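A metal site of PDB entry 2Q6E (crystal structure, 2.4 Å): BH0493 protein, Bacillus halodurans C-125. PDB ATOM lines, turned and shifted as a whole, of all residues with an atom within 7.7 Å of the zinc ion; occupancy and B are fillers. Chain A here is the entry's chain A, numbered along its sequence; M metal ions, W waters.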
ATOM      1  N   HIS A  26      14.397 -18.493  -4.278  1.00  0.00           N
ATOM      2  CA  HIS A  26      13.506 -17.498  -3.681  1.00  0.00           C
ATOM      3  C   HIS A  26      12.123 -18.064  -3.421  1.00  0.00           C
ATOM      4  O   HIS A  26      11.409 -18.432  -4.356  1.00  0.00           O
ATOM      5  CB  HIS A  26      13.358 -16.236  -4.538  1.00  0.00           C
ATOM      6  CG  HIS A  26      12.347 -15.284  -3.996  1.00  0.00           C
ATOM      7  ND1 HIS A  26      12.488 -14.663  -2.770  1.00  0.00           N
ATOM      8  CD2 HIS A  26      11.127 -14.904  -4.469  1.00  0.00           C
ATOM      9  CE1 HIS A  26      11.403 -13.949  -2.505  1.00  0.00           C
ATOM     10  NE2 HIS A  26      10.561 -14.085  -3.522  1.00  0.00           N
ATOM     11  N   THR A  27      11.749 -18.126  -2.153  1.00  0.00           N
ATOM     12  CA  THR A  27      10.443 -18.639  -1.755  1.00  0.00           C
ATOM     13  C   THR A  27       9.990 -17.957  -0.479  1.00  0.00           C
ATOM     14  O   THR A  27      10.729 -17.178   0.103  1.00  0.00           O
ATOM     15  CB  THR A  27      10.473 -20.154  -1.429  1.00  0.00           C
ATOM     16  OG1 THR A  27      11.029 -20.335  -0.117  1.00  0.00           O
ATOM     17  CG2 THR A  27      11.317 -20.907  -2.437  1.00  0.00           C
ATOM     18  N   HIS A  28       8.786 -18.273  -0.057  1.00  0.00           N
ATOM     19  CA  HIS A  28       8.240 -17.721   1.171  1.00  0.00           C
ATOM     20  C   HIS A  28       7.948 -18.868   2.125  1.00  0.00           C
ATOM     21  O   HIS A  28       6.974 -18.863   2.868  1.00  0.00           O
ATOM     22  CB  HIS A  28       6.985 -16.905   0.859  1.00  0.00           C
ATOM     23  CG  HIS A  28       7.272 -15.659   0.079  1.00  0.00           C
ATOM     24  ND1 HIS A  28       7.801 -14.522   0.662  1.00  0.00           N
ATOM     25  CD2 HIS A  28       7.157 -15.386  -1.239  1.00  0.00           C
ATOM     26  CE1 HIS A  28       8.007 -13.617  -0.267  1.00  0.00           C
ATOM     27  NE2 HIS A  28       7.635 -14.107  -1.437  1.00  0.00           N
ATOM     28  N   TYR A  50      -3.372 -15.738  -4.776  1.00  0.00           N
ATOM     29  CA  TYR A  50      -3.632 -15.845  -6.203  1.00  0.00           C
ATOM     30  C   TYR A  50      -5.088 -16.232  -6.447  1.00  0.00           C
ATOM     31  O   TYR A  50      -5.763 -15.643  -7.297  1.00  0.00           O
ATOM     32  CB  TYR A  50      -2.719 -16.891  -6.845  1.00  0.00           C
ATOM     33  CG  TYR A  50      -1.303 -16.453  -7.126  1.00  0.00           C
ATOM     34  CD1 TYR A  50      -0.600 -15.645  -6.224  1.00  0.00           C
ATOM     35  CD2 TYR A  50      -0.625 -16.914  -8.259  1.00  0.00           C
ATOM     36  CE1 TYR A  50       0.735 -15.314  -6.442  1.00  0.00           C
ATOM     37  CE2 TYR A  50       0.714 -16.585  -8.491  1.00  0.00           C
ATOM     38  CZ  TYR A  50       1.392 -15.788  -7.579  1.00  0.00           C
ATOM     39  OH  TYR A  50       2.712 -15.504  -7.785  1.00  0.00           O
ATOM     40  N   THR A 143      12.652 -16.232   2.675  1.00  0.00           N
ATOM     41  CA  THR A 143      12.550 -14.786   2.714  1.00  0.00           C
ATOM     42  C   THR A 143      12.474 -14.488   4.210  1.00  0.00           C
ATOM     43  O   THR A 143      11.433 -14.698   4.837  1.00  0.00           O
ATOM     44  CB  THR A 143      11.282 -14.279   2.013  1.00  0.00           C
ATOM     45  OG1 THR A 143      11.374 -14.555   0.614  1.00  0.00           O
ATOM     46  CG2 THR A 143      11.124 -12.789   2.221  1.00  0.00           C
ATOM     47  N   SER A 223      11.860  -5.507  -2.738  1.00  0.00           N
ATOM     48  CA  SER A 223      10.954  -5.443  -3.881  1.00  0.00           C
ATOM     49  C   SER A 223      10.770  -3.938  -4.106  1.00  0.00           C
ATOM     50  O   SER A 223      10.637  -3.175  -3.150  1.00  0.00           O
ATOM     51  CB  SER A 223       9.622  -6.143  -3.592  1.00  0.00           C
ATOM     52  OG  SER A 223       8.924  -5.541  -2.526  1.00  0.00           O
ATOM     53  N   MET A 258      13.719  -6.988  -6.866  1.00  0.00           N
ATOM     54  CA  MET A 258      12.519  -7.511  -7.521  1.00  0.00           C
ATOM     55  C   MET A 258      11.734  -6.240  -7.841  1.00  0.00           C
ATOM     56  O   MET A 258      11.015  -5.692  -7.002  1.00  0.00           O
ATOM     57  CB  MET A 258      11.774  -8.434  -6.558  1.00  0.00           C
ATOM     58  CG  MET A 258      12.744  -9.299  -5.752  1.00  0.00           C
ATOM     59  SD  MET A 258      12.085 -10.895  -5.267  1.00  0.00           S
ATOM     60  CE  MET A 258      11.062 -10.436  -3.864  1.00  0.00           C
ATOM     61  N   TRP A 325       8.794 -14.060 -12.406  1.00  0.00           N
ATOM     62  CA  TRP A 325       8.101 -13.590 -11.219  1.00  0.00           C
ATOM     63  C   TRP A 325       6.626 -13.199 -11.258  1.00  0.00           C
ATOM     64  O   TRP A 325       6.184 -12.425 -12.106  1.00  0.00           O
ATOM     65  CB  TRP A 325       8.925 -12.432 -10.648  1.00  0.00           C
ATOM     66  CG  TRP A 325       8.449 -11.887  -9.341  1.00  0.00           C
ATOM     67  CD1 TRP A 325       7.973 -12.583  -8.283  1.00  0.00           C
ATOM     68  CD2 TRP A 325       8.511 -10.516  -8.925  1.00  0.00           C
ATOM     69  NE1 TRP A 325       7.739 -11.740  -7.220  1.00  0.00           N
ATOM     70  CE2 TRP A 325       8.059 -10.463  -7.594  1.00  0.00           C
ATOM     71  CE3 TRP A 325       8.901  -9.319  -9.557  1.00  0.00           C
ATOM     72  CZ2 TRP A 325       7.998  -9.273  -6.863  1.00  0.00           C
ATOM     73  CZ3 TRP A 325       8.833  -8.130  -8.842  1.00  0.00           C
ATOM     74  CH2 TRP A 325       8.389  -8.120  -7.502  1.00  0.00           C
ATOM     75  N   TRP A 326       5.873 -13.766 -10.313  1.00  0.00           N
ATOM     76  CA  TRP A 326       4.462 -13.441 -10.101  1.00  0.00           C
ATOM     77  C   TRP A 326       3.571 -13.464 -11.344  1.00  0.00           C
ATOM     78  O   TRP A 326       3.216 -14.525 -11.871  1.00  0.00           O
ATOM     79  CB  TRP A 326       4.452 -12.053  -9.463  1.00  0.00           C
ATOM     80  CG  TRP A 326       3.327 -11.728  -8.564  1.00  0.00           C
ATOM     81  CD1 TRP A 326       2.066 -12.245  -8.591  1.00  0.00           C
ATOM     82  CD2 TRP A 326       3.331 -10.716  -7.561  1.00  0.00           C
ATOM     83  NE1 TRP A 326       1.283 -11.600  -7.659  1.00  0.00           N
ATOM     84  CE2 TRP A 326       2.038 -10.655  -7.012  1.00  0.00           C
ATOM     85  CE3 TRP A 326       4.317  -9.839  -7.076  1.00  0.00           C
ATOM     86  CZ2 TRP A 326       1.696  -9.755  -6.003  1.00  0.00           C
ATOM     87  CZ3 TRP A 326       3.975  -8.939  -6.067  1.00  0.00           C
ATOM     88  CH2 TRP A 326       2.668  -8.911  -5.546  1.00  0.00           C
ATOM     89  N   HIS A 353      12.263 -19.702 -10.266  1.00  0.00           N
ATOM     90  CA  HIS A 353      12.221 -19.823  -8.816  1.00  0.00           C
ATOM     91  C   HIS A 353      10.728 -20.011  -8.576  1.00  0.00           C
ATOM     92  O   HIS A 353       9.918 -19.645  -9.439  1.00  0.00           O
ATOM     93  CB  HIS A 353      12.735 -18.564  -8.094  1.00  0.00           C
ATOM     94  CG  HIS A 353      11.861 -17.362  -8.248  1.00  0.00           C
ATOM     95  ND1 HIS A 353      11.859 -16.565  -9.372  1.00  0.00           N
ATOM     96  CD2 HIS A 353      10.946 -16.809  -7.411  1.00  0.00           C
ATOM     97  CE1 HIS A 353      10.990 -15.583  -9.227  1.00  0.00           C
ATOM     98  NE2 HIS A 353      10.419 -15.709  -8.040  1.00  0.00           N
ATOM     99  N   SER A 354      10.348 -20.595  -7.444  1.00  0.00           N
ATOM    100  CA  SER A 354       8.925 -20.860  -7.201  1.00  0.00           C
ATOM    101  C   SER A 354       8.131 -19.752  -6.530  1.00  0.00           C
ATOM    102  O   SER A 354       6.960 -19.539  -6.857  1.00  0.00           O
ATOM    103  CB  SER A 354       8.757 -22.126  -6.364  1.00  0.00           C
ATOM    104  OG  SER A 354       9.144 -21.895  -5.011  1.00  0.00           O
ATOM    105  N   ASP A 355       8.745 -19.053  -5.582  1.00  0.00           N
ATOM    106  CA  ASP A 355       8.064 -17.992  -4.834  1.00  0.00           C
ATOM    107  C   ASP A 355       6.955 -18.631  -3.997  1.00  0.00           C
ATOM    108  O   ASP A 355       5.997 -17.955  -3.594  1.00  0.00           O
ATOM    109  CB  ASP A 355       7.442 -16.980  -5.801  1.00  0.00           C
ATOM    110  CG  ASP A 355       7.743 -15.544  -5.420  1.00  0.00           C
ATOM    111  OD1 ASP A 355       7.335 -15.086  -4.325  1.00  0.00           O
ATOM    112  OD2 ASP A 355       8.398 -14.857  -6.227  1.00  0.00           O
ATOM    113  N   ALA A 356       7.081 -19.925  -3.735  1.00  0.00           N
ATOM    114  CA  ALA A 356       6.072 -20.659  -2.965  1.00  0.00           C
ATOM    115  C   ALA A 356       5.796 -20.066  -1.589  1.00  0.00           C
ATOM    116  O   ALA A 356       6.724 -19.701  -0.862  1.00  0.00           O
ATOM    117  CB  ALA A 356       6.487 -22.127  -2.825  1.00  0.00           C
ATOM    118  N   ARG A 357       4.514 -19.947  -1.261  1.00  0.00           N
ATOM    119  CA  ARG A 357       4.063 -19.413   0.032  1.00  0.00           C
ATOM    120  C   ARG A 357       3.518 -20.571   0.853  1.00  0.00           C
ATOM    121  O   ARG A 357       3.500 -20.533   2.082  1.00  0.00           O
ATOM    122  CB  ARG A 357       2.950 -18.389  -0.172  1.00  0.00           C
ATOM    123  CG  ARG A 357       3.457 -17.034  -0.613  1.00  0.00           C
ATOM    124  CD  ARG A 357       2.307 -16.081  -0.919  1.00  0.00           C
ATOM    125  NE  ARG A 357       2.784 -14.716  -1.065  1.00  0.00           N
ATOM    126  CZ  ARG A 357       3.290 -14.001  -0.060  1.00  0.00           C
ATOM    127  NH1 ARG A 357       3.376 -14.516   1.158  1.00  0.00           N
ATOM    128  NH2 ARG A 357       3.720 -12.757  -0.272  1.00  0.00           N
HETATM  129 ZN    ZN M   1       8.404 -13.547  -3.409  1.00  0.00          ZN
HETATM  130  O   HOH W   1       8.123 -11.385  -3.453  1.00  0.00           O
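The nearest printed residue that does not touch the zinc ion is Met 258 (4.1 Å).
NE1 of Trp 325 sits close to OD2 of Asp 355, at 3.3 Å. The side-chain carboxylate (OD2) of Asp 355 sits at hydrogen-bond distance from a ring nitrogen (NE2) of His 353, 2.8 Å away. The backbone NH (N) of His 28 sits at hydrogen-bond distance from the backbone carbonyl oxygen (O) of Ala 356 (2.6 Å).
The zinc ion is bound by OD1 of Asp 355 (2.1 Å), water W1 (2.2 Å), NE2 of His 28 (2.2 Å) and NE2 of His 26 (2.2 Å).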
